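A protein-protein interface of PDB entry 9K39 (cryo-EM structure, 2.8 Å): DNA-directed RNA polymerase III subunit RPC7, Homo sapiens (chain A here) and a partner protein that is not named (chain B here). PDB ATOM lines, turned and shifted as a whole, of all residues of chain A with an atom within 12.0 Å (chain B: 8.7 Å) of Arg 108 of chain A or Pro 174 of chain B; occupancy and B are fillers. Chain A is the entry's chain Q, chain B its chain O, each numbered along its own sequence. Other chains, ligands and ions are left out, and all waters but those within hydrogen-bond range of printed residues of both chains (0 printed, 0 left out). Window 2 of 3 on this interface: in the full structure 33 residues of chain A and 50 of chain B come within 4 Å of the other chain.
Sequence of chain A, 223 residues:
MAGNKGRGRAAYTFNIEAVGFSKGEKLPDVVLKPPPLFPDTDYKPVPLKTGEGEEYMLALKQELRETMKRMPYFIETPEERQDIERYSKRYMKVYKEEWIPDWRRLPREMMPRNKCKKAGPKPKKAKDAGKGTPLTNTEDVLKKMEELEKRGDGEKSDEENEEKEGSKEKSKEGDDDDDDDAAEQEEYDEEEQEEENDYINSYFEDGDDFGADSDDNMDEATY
The guanidinium group (NH1) of Arg 113 of chain A sits at hydrogen-bond distance from the backbone carbonyl oxygen (O) of Arg 108 of chain A (3.1 Å).
OD2 of Asp 102 of chain A is in salt-bridge range of NH2 of Arg 104 of chain A (2.8 Å).
NH1 of Arg 113 of chain A sits at hydrogen-bond distance from O of Met 111 of chain A (2.7 Å).
Among the printed residues, pairs that only touch across the chains: Glu 109 of chain A with Val 73 of chain B (3.0 Å), Arg 105 of chain A with Pro 178 of chain B (3.1 Å), Pro 107 of chain A with Pro 176 of chain B (3.1 Å), Arg 104 of chain A with Pro 178 of chain B (3.2 Å), Met 110 of chain A with Leu 36 of chain B (3.3 Å), Glu 109 of chain A with Lys 51 of chain B (3.4 Å), Pro 107 of chain A with Tyr 65 of chain B (3.5 Å), Met 111 of chain A with Lys 51 of chain B (3.8 Å), Glu 109 of chain A with Tyr 75 of chain B (3.9 Å), Pro 107 of chain A with Ala 177 of chain B (3.9 Å), Met 110 of chain A with Lys 51 of chain B (3.9 Å) and Glu 109 of chain A with Leu 36 of chain B (3.99 Å).
Of the printed residues of chain B, Pro 107 of chain A touches Tyr 65, Pro 176 and Ala 177.
Of chain B, only Pro 174, Pro 175 and Pro 176 come within 4 Å of Arg 108 of chain A.
Of the printed residues of chain B, Glu 109 of chain A touches Leu 36, Lys 51, Val 73 and Tyr 75.
Gly 71 of chain B touches none of the printed residues of chain A.
Ser 169 of chain B touches none of the printed residues of chain A.
No residue of chain A comes within 4 Å of Gly 172 of chain B.
No residue of chain A comes within 4 Å of Pro 173 of chain B.
Of chain A, only Arg 108 comes within 4 Å of Pro 174 of chain B.
Pro 175 of chain B touches just one residue of chain A: Arg 108 (3.1 Å).
Ala 177 of chain B touches just one residue of chain A: Pro 107.
The nearest residue of chain A that does not touch Pro 174 of chain B is Met 111 of chain A (9.1 Å).
O of Pro 174 of chain B sits at hydrogen-bond distance from NH2 of Arg 108 of chain A (2.4 Å).
O of Arg 105 of chain A sits close to OH of Tyr 65 of chain B.
NH2 of Arg 108 of chain A is in hydrogen-bond range of O of Pro 175 of chain B (3.1 Å).
The guanidinium group (NH2) of Arg 113 of chain A sits close to the side-chain amino group (NZ) of Lys 51 of chain B.
The side-chain hydroxyl (OH) of Tyr 75 of chain B is in hydrogen-bond range of the side-chain sulfur (SD) of Met 110 of chain A, at 2.7 Å.
O of Pro 176 of chain B is in hydrogen-bond range of N of Arg 108 of chain A (3.3 Å).
Of the 13 printed residues of chain A, 8 touch a printed residue of chain B.
Hydrophobic or aromatic side chains of chain A that line the printed part of chain B: Pro 107 and Met 110.
Of the 17 printed residues of chain B, 10 touch a printed residue of chain A.
Printed residues of chain B that touch a printed residue of chain A: Leu 36, Lys 51, Tyr 65, Val 73, Tyr 75, Pro 174, Pro 175, Pro 176, Ala 177 and Pro 178.
Hydrophobic or aromatic side chains of chain B within 4 Å of the printed part of chain A: Leu 36, Tyr 65, Val 73, Tyr 75, Pro 174, Pro 176, Ala 177 and Pro 178.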
ATOM      1  N   PRO A 101       0.923   7.639 -15.532  1.00  0.00           N
ATOM      2  CA  PRO A 101       1.226   8.794 -16.383  1.00  0.00           C
ATOM      3  C   PRO A 101       1.073  10.102 -15.624  1.00  0.00           C
ATOM      4  O   PRO A 101       0.262  10.225 -14.703  1.00  0.00           O
ATOM      5  CB  PRO A 101       0.197   8.686 -17.515  1.00  0.00           C
ATOM      6  CG  PRO A 101      -0.290   7.266 -17.469  1.00  0.00           C
ATOM      7  CD  PRO A 101      -0.233   6.874 -16.029  1.00  0.00           C
ATOM      8  N   ASP A 102       1.870  11.089 -16.025  1.00  0.00           N
ATOM      9  CA  ASP A 102       1.832  12.412 -15.414  1.00  0.00           C
ATOM     10  C   ASP A 102       0.649  13.173 -16.000  1.00  0.00           C
ATOM     11  O   ASP A 102       0.709  13.675 -17.125  1.00  0.00           O
ATOM     12  CB  ASP A 102       3.144  13.154 -15.650  1.00  0.00           C
ATOM     13  CG  ASP A 102       3.337  14.324 -14.703  1.00  0.00           C
ATOM     14  OD1 ASP A 102       2.328  14.909 -14.253  1.00  0.00           O
ATOM     15  OD2 ASP A 102       4.503  14.659 -14.404  1.00  0.00           O
ATOM     16  N   TRP A 103      -0.440  13.255 -15.233  1.00  0.00           N
ATOM     17  CA  TRP A 103      -1.654  13.914 -15.703  1.00  0.00           C
ATOM     18  C   TRP A 103      -1.518  15.430 -15.779  1.00  0.00           C
ATOM     19  O   TRP A 103      -2.424  16.087 -16.301  1.00  0.00           O
ATOM     20  CB  TRP A 103      -2.828  13.542 -14.798  1.00  0.00           C
ATOM     21  CG  TRP A 103      -2.947  12.068 -14.565  1.00  0.00           C
ATOM     22  CD1 TRP A 103      -2.663  11.393 -13.414  1.00  0.00           C
ATOM     23  CD2 TRP A 103      -3.365  11.078 -15.516  1.00  0.00           C
ATOM     24  NE1 TRP A 103      -2.886  10.048 -13.586  1.00  0.00           N
ATOM     25  CE2 TRP A 103      -3.317   9.829 -14.868  1.00  0.00           C
ATOM     26  CE3 TRP A 103      -3.780  11.131 -16.851  1.00  0.00           C
ATOM     27  CZ2 TRP A 103      -3.668   8.642 -15.509  1.00  0.00           C
ATOM     28  CZ3 TRP A 103      -4.127   9.953 -17.485  1.00  0.00           C
ATOM     29  CH2 TRP A 103      -4.068   8.724 -16.814  1.00  0.00           C
ATOM     30  N   ARG A 104      -0.423  15.998 -15.269  1.00  0.00           N
ATOM     31  CA  ARG A 104      -0.222  17.440 -15.380  1.00  0.00           C
ATOM     32  C   ARG A 104       0.079  17.842 -16.818  1.00  0.00           C
ATOM     33  O   ARG A 104      -0.467  18.833 -17.321  1.00  0.00           O
ATOM     34  CB  ARG A 104       0.908  17.885 -14.449  1.00  0.00           C
ATOM     35  CG  ARG A 104       0.657  17.577 -12.982  1.00  0.00           C
ATOM     36  CD  ARG A 104       1.880  17.895 -12.141  1.00  0.00           C
ATOM     37  NE  ARG A 104       3.042  17.111 -12.552  1.00  0.00           N
ATOM     38  CZ  ARG A 104       4.237  17.194 -11.975  1.00  0.00           C
ATOM     39  NH1 ARG A 104       4.431  18.024 -10.963  1.00  0.00           N
ATOM     40  NH2 ARG A 104       5.239  16.443 -12.415  1.00  0.00           N
ATOM     41  N   ARG A 105       0.941  17.084 -17.498  1.00  0.00           N
ATOM     42  CA  ARG A 105       1.265  17.379 -18.889  1.00  0.00           C
ATOM     43  C   ARG A 105       0.195  16.845 -19.832  1.00  0.00           C
ATOM     44  O   ARG A 105      -0.154  17.503 -20.818  1.00  0.00           O
ATOM     45  CB  ARG A 105       2.631  16.789 -19.243  1.00  0.00           C
ATOM     46  CG  ARG A 105       3.747  17.193 -18.296  1.00  0.00           C
ATOM     47  CD  ARG A 105       4.999  16.359 -18.528  1.00  0.00           C
ATOM     48  NE  ARG A 105       5.557  16.558 -19.863  1.00  0.00           N
ATOM     49  CZ  ARG A 105       6.512  17.434 -20.146  1.00  0.00           C
ATOM     50  NH1 ARG A 105       7.021  18.199 -19.192  1.00  0.00           N
ATOM     51  NH2 ARG A 105       6.961  17.549 -21.391  1.00  0.00           N
ATOM     52  N   LEU A 106      -0.327  15.656 -19.550  1.00  0.00           N
ATOM     53  CA  LEU A 106      -1.348  15.065 -20.399  1.00  0.00           C
ATOM     54  C   LEU A 106      -2.687  15.767 -20.178  1.00  0.00           C
ATOM     55  O   LEU A 106      -3.049  16.071 -19.036  1.00  0.00           O
ATOM     56  CB  LEU A 106      -1.478  13.573 -20.101  1.00  0.00           C
ATOM     57  CG  LEU A 106      -2.330  12.698 -21.019  1.00  0.00           C
ATOM     58  CD1 LEU A 106      -1.740  12.644 -22.419  1.00  0.00           C
ATOM     59  CD2 LEU A 106      -2.453  11.300 -20.437  1.00  0.00           C
ATOM     60  N   PRO A 107      -3.440  16.047 -21.243  1.00  0.00           N
ATOM     61  CA  PRO A 107      -4.757  16.673 -21.075  1.00  0.00           C
ATOM     62  C   PRO A 107      -5.710  15.801 -20.272  1.00  0.00           C
ATOM     63  O   PRO A 107      -5.485  14.606 -20.062  1.00  0.00           O
ATOM     64  CB  PRO A 107      -5.250  16.855 -22.516  1.00  0.00           C
ATOM     65  CG  PRO A 107      -4.005  16.912 -23.333  1.00  0.00           C
ATOM     66  CD  PRO A 107      -3.032  15.987 -22.657  1.00  0.00           C
ATOM     67  N   ARG A 108      -6.800  16.426 -19.820  1.00  0.00           N
ATOM     68  CA  ARG A 108      -7.736  15.764 -18.915  1.00  0.00           C
ATOM     69  C   ARG A 108      -8.519  14.642 -19.588  1.00  0.00           C
ATOM     70  O   ARG A 108      -9.098  13.804 -18.887  1.00  0.00           O
ATOM     71  CB  ARG A 108      -8.712  16.784 -18.330  1.00  0.00           C
ATOM     72  CG  ARG A 108      -9.719  17.324 -19.337  1.00  0.00           C
ATOM     73  CD  ARG A 108     -10.878  18.023 -18.643  1.00  0.00           C
ATOM     74  NE  ARG A 108     -10.478  19.282 -18.022  1.00  0.00           N
ATOM     75  CZ  ARG A 108     -10.627  20.475 -18.589  1.00  0.00           C
ATOM     76  NH1 ARG A 108     -11.175  20.575 -19.792  1.00  0.00           N
ATOM     77  NH2 ARG A 108     -10.237  21.568 -17.949  1.00  0.00           N
ATOM     78  N   GLU A 109      -8.560  14.607 -20.920  1.00  0.00           N
ATOM     79  CA  GLU A 109      -9.433  13.670 -21.616  1.00  0.00           C
ATOM     80  C   GLU A 109      -8.952  12.224 -21.546  1.00  0.00           C
ATOM     81  O   GLU A 109      -9.706  11.328 -21.939  1.00  0.00           O
ATOM     82  CB  GLU A 109      -9.588  14.088 -23.081  1.00  0.00           C
ATOM     83  CG  GLU A 109     -10.254  15.442 -23.271  1.00  0.00           C
ATOM     84  CD  GLU A 109     -10.453  15.792 -24.734  1.00  0.00           C
ATOM     85  OE1 GLU A 109     -10.077  14.973 -25.598  1.00  0.00           O
ATOM     86  OE2 GLU A 109     -10.986  16.885 -25.019  1.00  0.00           O
ATOM     87  N   MET A 110      -7.737  11.971 -21.065  1.00  0.00           N
ATOM     88  CA  MET A 110      -7.186  10.620 -21.035  1.00  0.00           C
ATOM     89  C   MET A 110      -7.157  10.012 -19.636  1.00  0.00           C
ATOM     90  O   MET A 110      -6.541   8.959 -19.448  1.00  0.00           O
ATOM     91  CB  MET A 110      -5.781  10.606 -21.638  1.00  0.00           C
ATOM     92  CG  MET A 110      -5.753  10.572 -23.159  1.00  0.00           C
ATOM     93  SD  MET A 110      -6.488  12.036 -23.908  1.00  0.00           S
ATOM     94  CE  MET A 110      -5.422  13.312 -23.253  1.00  0.00           C
ATOM     95  N   MET A 111      -7.799  10.640 -18.656  1.00  0.00           N
ATOM     96  CA  MET A 111      -7.870  10.037 -17.333  1.00  0.00           C
ATOM     97  C   MET A 111      -8.872   8.886 -17.333  1.00  0.00           C
ATOM     98  O   MET A 111      -9.920   8.971 -17.980  1.00  0.00           O
ATOM     99  CB  MET A 111      -8.261  11.071 -16.278  1.00  0.00           C
ATOM    100  CG  MET A 111      -7.076  11.778 -15.636  1.00  0.00           C
ATOM    101  SD  MET A 111      -6.780  13.426 -16.298  1.00  0.00           S
ATOM    102  CE  MET A 111      -8.174  14.312 -15.606  1.00  0.00           C
ATOM    103  N   PRO A 112      -8.576   7.791 -16.629  1.00  0.00           N
ATOM    104  CA  PRO A 112      -9.501   6.647 -16.637  1.00  0.00           C
ATOM    105  C   PRO A 112     -10.813   6.917 -15.921  1.00  0.00           C
ATOM    106  O   PRO A 112     -11.859   6.431 -16.371  1.00  0.00           O
ATOM    107  CB  PRO A 112      -8.697   5.542 -15.933  1.00  0.00           C
ATOM    108  CG  PRO A 112      -7.267   5.996 -15.979  1.00  0.00           C
ATOM    109  CD  PRO A 112      -7.326   7.489 -15.911  1.00  0.00           C
ATOM    110  N   ARG A 113     -10.787   7.678 -14.829  1.00  0.00           N
ATOM    111  CA  ARG A 113     -11.966   7.914 -13.993  1.00  0.00           C
ATOM    112  C   ARG A 113     -12.622   6.602 -13.566  1.00  0.00           C
ATOM    113  O   ARG A 113     -13.188   6.507 -12.478  1.00  0.00           O
ATOM    114  CB  ARG A 113     -12.989   8.797 -14.716  1.00  0.00           C
ATOM    115  CG  ARG A 113     -12.640  10.279 -14.731  1.00  0.00           C
ATOM    116  CD  ARG A 113     -11.855  10.662 -15.974  1.00  0.00           C
ATOM    117  NE  ARG A 113     -12.672  10.579 -17.182  1.00  0.00           N
ATOM    118  CZ  ARG A 113     -12.253  10.939 -18.393  1.00  0.00           C
ATOM    119  NH1 ARG A 113     -11.024  11.410 -18.558  1.00  0.00           N
ATOM    120  NH2 ARG A 113     -13.063  10.830 -19.436  1.00  0.00           N
ATOM    121  N   LEU B  36     -10.106  13.123 -30.239  1.00  0.00           N
ATOM    122  CA  LEU B  36     -10.089  11.786 -29.653  1.00  0.00           C
ATOM    123  C   LEU B  36     -11.343  10.994 -30.018  1.00  0.00           C
ATOM    124  O   LEU B  36     -11.267   9.790 -30.287  1.00  0.00           O
ATOM    125  CB  LEU B  36      -9.937  11.894 -28.133  1.00  0.00           C
ATOM    126  CG  LEU B  36      -9.530  10.655 -27.332  1.00  0.00           C
ATOM    127  CD1 LEU B  36      -8.820  11.078 -26.058  1.00  0.00           C
ATOM    128  CD2 LEU B  36     -10.732   9.786 -26.990  1.00  0.00           C
ATOM    129  N   LYS B  51      -7.580   5.914 -25.078  1.00  0.00           N
ATOM    130  CA  LYS B  51      -6.881   6.784 -24.135  1.00  0.00           C
ATOM    131  C   LYS B  51      -5.528   6.203 -23.744  1.00  0.00           C
ATOM    132  O   LYS B  51      -4.524   6.925 -23.693  1.00  0.00           O
ATOM    133  CB  LYS B  51      -7.745   7.014 -22.896  1.00  0.00           C
ATOM    134  CG  LYS B  51      -9.069   7.701 -23.176  1.00  0.00           C
ATOM    135  CD  LYS B  51      -9.926   7.767 -21.924  1.00  0.00           C
ATOM    136  CE  LYS B  51     -11.284   8.384 -22.213  1.00  0.00           C
ATOM    137  NZ  LYS B  51     -12.148   8.417 -21.003  1.00  0.00           N
ATOM    138  N   TYR B  65      -0.280  16.826 -28.878  1.00  0.00           N
ATOM    139  CA  TYR B  65      -1.644  17.318 -28.750  1.00  0.00           C
ATOM    140  C   TYR B  65      -1.647  18.839 -28.823  1.00  0.00           C
ATOM    141  O   TYR B  65      -0.817  19.502 -28.197  1.00  0.00           O
ATOM    142  CB  TYR B  65      -2.289  16.846 -27.440  1.00  0.00           C
ATOM    143  CG  TYR B  65      -1.447  17.076 -26.202  1.00  0.00           C
ATOM    144  CD1 TYR B  65      -0.525  16.126 -25.782  1.00  0.00           C
ATOM    145  CD2 TYR B  65      -1.583  18.237 -25.452  1.00  0.00           C
ATOM    146  CE1 TYR B  65       0.245  16.330 -24.652  1.00  0.00           C
ATOM    147  CE2 TYR B  65      -0.817  18.448 -24.320  1.00  0.00           C
ATOM    148  CZ  TYR B  65       0.094  17.493 -23.925  1.00  0.00           C
ATOM    149  OH  TYR B  65       0.860  17.698 -22.801  1.00  0.00           O
ATOM    150  N   GLY B  71     -11.859  25.016 -27.861  1.00  0.00           N
ATOM    151  CA  GLY B  71     -11.133  24.277 -26.850  1.00  0.00           C
ATOM    152  C   GLY B  71     -10.961  22.800 -27.125  1.00  0.00           C
ATOM    153  O   GLY B  71     -10.678  22.039 -26.195  1.00  0.00           O
ATOM    154  N   VAL B  73      -9.134  19.387 -28.450  1.00  0.00           N
ATOM    155  CA  VAL B  73      -7.762  18.897 -28.503  1.00  0.00           C
ATOM    156  C   VAL B  73      -7.632  17.945 -29.681  1.00  0.00           C
ATOM    157  O   VAL B  73      -8.471  17.056 -29.871  1.00  0.00           O
ATOM    158  CB  VAL B  73      -7.362  18.216 -27.182  1.00  0.00           C
ATOM    159  CG1 VAL B  73      -8.425  17.217 -26.745  1.00  0.00           C
ATOM    160  CG2 VAL B  73      -6.004  17.536 -27.318  1.00  0.00           C
ATOM    161  N   TYR B  75      -4.853  15.368 -31.797  1.00  0.00           N
ATOM    162  CA  TYR B  75      -3.622  14.604 -31.670  1.00  0.00           C
ATOM    163  C   TYR B  75      -3.042  14.338 -33.052  1.00  0.00           C
ATOM    164  O   TYR B  75      -3.737  13.820 -33.933  1.00  0.00           O
ATOM    165  CB  TYR B  75      -3.872  13.280 -30.942  1.00  0.00           C
ATOM    166  CG  TYR B  75      -4.540  13.438 -29.593  1.00  0.00           C
ATOM    167  CD1 TYR B  75      -3.791  13.665 -28.447  1.00  0.00           C
ATOM    168  CD2 TYR B  75      -5.922  13.356 -29.469  1.00  0.00           C
ATOM    169  CE1 TYR B  75      -4.398  13.809 -27.214  1.00  0.00           C
ATOM    170  CE2 TYR B  75      -6.537  13.499 -28.241  1.00  0.00           C
ATOM    171  CZ  TYR B  75      -5.772  13.726 -27.118  1.00  0.00           C
ATOM    172  OH  TYR B  75      -6.382  13.868 -25.892  1.00  0.00           O
ATOM    173  N   THR B 166       0.389  27.247 -13.622  1.00  0.00           N
ATOM    174  CA  THR B 166      -1.048  27.484 -13.737  1.00  0.00           C
ATOM    175  C   THR B 166      -1.477  28.703 -12.928  1.00  0.00           C
ATOM    176  O   THR B 166      -2.416  29.410 -13.312  1.00  0.00           O
ATOM    177  CB  THR B 166      -1.822  26.245 -13.290  1.00  0.00           C
ATOM    178  OG1 THR B 166      -1.513  25.951 -11.923  1.00  0.00           O
ATOM    179  CG2 THR B 166      -1.453  25.048 -14.156  1.00  0.00           C
ATOM    180  N   SER B 169      -0.096  31.943 -14.967  1.00  0.00           N
ATOM    181  CA  SER B 169      -0.650  32.041 -16.316  1.00  0.00           C
ATOM    182  C   SER B 169      -2.128  31.676 -16.266  1.00  0.00           C
ATOM    183  O   SER B 169      -2.487  30.497 -16.186  1.00  0.00           O
ATOM    184  CB  SER B 169       0.114  31.140 -17.280  1.00  0.00           C
ATOM    185  OG  SER B 169       0.016  29.781 -16.896  1.00  0.00           O
ATOM    186  N   ASP B 170      -2.987  32.698 -16.310  1.00  0.00           N
ATOM    187  CA  ASP B 170      -4.439  32.556 -16.370  1.00  0.00           C
ATOM    188  C   ASP B 170      -4.967  31.736 -15.198  1.00  0.00           C
ATOM    189  O   ASP B 170      -5.409  30.595 -15.391  1.00  0.00           O
ATOM    190  CB  ASP B 170      -4.859  31.917 -17.696  1.00  0.00           C
ATOM    191  CG  ASP B 170      -6.351  32.021 -17.949  1.00  0.00           C
ATOM    192  OD1 ASP B 170      -7.046  32.710 -17.171  1.00  0.00           O
ATOM    193  OD2 ASP B 170      -6.832  31.411 -18.928  1.00  0.00           O
ATOM    194  N   PRO B 171      -4.938  32.268 -13.975  1.00  0.00           N
ATOM    195  CA  PRO B 171      -5.494  31.523 -12.838  1.00  0.00           C
ATOM    196  C   PRO B 171      -7.015  31.482 -12.907  1.00  0.00           C
ATOM    197  O   PRO B 171      -7.674  32.518 -13.030  1.00  0.00           O
ATOM    198  CB  PRO B 171      -5.004  32.313 -11.620  1.00  0.00           C
ATOM    199  CG  PRO B 171      -4.834  33.704 -12.132  1.00  0.00           C
ATOM    200  CD  PRO B 171      -4.395  33.576 -13.568  1.00  0.00           C
ATOM    201  N   GLY B 172      -7.569  30.274 -12.832  1.00  0.00           N
ATOM    202  CA  GLY B 172      -8.999  30.095 -12.890  1.00  0.00           C
ATOM    203  C   GLY B 172      -9.397  28.751 -13.463  1.00  0.00           C
ATOM    204  O   GLY B 172      -8.930  27.696 -13.019  1.00  0.00           O
ATOM    205  N   PRO B 173     -10.280  28.763 -14.458  1.00  0.00           N
ATOM    206  CA  PRO B 173     -10.741  27.510 -15.066  1.00  0.00           C
ATOM    207  C   PRO B 173      -9.599  26.781 -15.750  1.00  0.00           C
ATOM    208  O   PRO B 173      -8.829  27.386 -16.511  1.00  0.00           O
ATOM    209  CB  PRO B 173     -11.793  27.976 -16.085  1.00  0.00           C
ATOM    210  CG  PRO B 173     -12.201  29.342 -15.623  1.00  0.00           C
ATOM    211  CD  PRO B 173     -10.968  29.937 -15.017  1.00  0.00           C
ATOM    212  N   PRO B 174      -9.456  25.482 -15.507  1.00  0.00           N
ATOM    213  CA  PRO B 174      -8.377  24.721 -16.140  1.00  0.00           C
ATOM    214  C   PRO B 174      -8.707  24.416 -17.590  1.00  0.00           C
ATOM    215  O   PRO B 174      -9.824  23.981 -17.908  1.00  0.00           O
ATOM    216  CB  PRO B 174      -8.311  23.438 -15.300  1.00  0.00           C
ATOM    217  CG  PRO B 174      -9.696  23.276 -14.772  1.00  0.00           C
ATOM    218  CD  PRO B 174     -10.229  24.667 -14.553  1.00  0.00           C
ATOM    219  N   PRO B 175      -7.764  24.637 -18.501  1.00  0.00           N
ATOM    220  CA  PRO B 175      -8.014  24.346 -19.915  1.00  0.00           C
ATOM    221  C   PRO B 175      -8.009  22.852 -20.171  1.00  0.00           C
ATOM    222  O   PRO B 175      -7.480  22.077 -19.360  1.00  0.00           O
ATOM    223  CB  PRO B 175      -6.840  25.039 -20.625  1.00  0.00           C
ATOM    224  CG  PRO B 175      -5.745  25.025 -19.615  1.00  0.00           C
ATOM    225  CD  PRO B 175      -6.417  25.189 -18.274  1.00  0.00           C
ATOM    226  N   PRO B 176      -8.603  22.403 -21.281  1.00  0.00           N
ATOM    227  CA  PRO B 176      -8.552  20.964 -21.600  1.00  0.00           C
ATOM    228  C   PRO B 176      -7.138  20.440 -21.759  1.00  0.00           C
ATOM    229  O   PRO B 176      -6.859  19.291 -21.394  1.00  0.00           O
ATOM    230  CB  PRO B 176      -9.350  20.870 -22.909  1.00  0.00           C
ATOM    231  CG  PRO B 176     -10.233  22.076 -22.905  1.00  0.00           C
ATOM    232  CD  PRO B 176      -9.438  23.156 -22.234  1.00  0.00           C
ATOM    233  N   ALA B 177      -6.232  21.253 -22.298  1.00  0.00           N
ATOM    234  CA  ALA B 177      -4.835  20.884 -22.440  1.00  0.00           C
ATOM    235  C   ALA B 177      -3.960  21.950 -21.799  1.00  0.00           C
ATOM    236  O   ALA B 177      -4.214  23.151 -21.970  1.00  0.00           O
ATOM    237  CB  ALA B 177      -4.452  20.710 -23.917  1.00  0.00           C
ATOM    238  N   PRO B 178      -2.924  21.552 -21.056  1.00  0.00           N
ATOM    239  CA  PRO B 178      -2.075  22.545 -20.378  1.00  0.00           C
ATOM    240  C   PRO B 178      -1.201  23.359 -21.317  1.00  0.00           C
ATOM    241  O   PRO B 178      -0.551  24.304 -20.851  1.00  0.00           O
ATOM    242  CB  PRO B 178      -1.224  21.690 -19.430  1.00  0.00           C
ATOM    243  CG  PRO B 178      -1.202  20.338 -20.060  1.00  0.00           C
ATOM    244  CD  PRO B 178      -2.529  20.167 -20.739  1.00  0.00           C
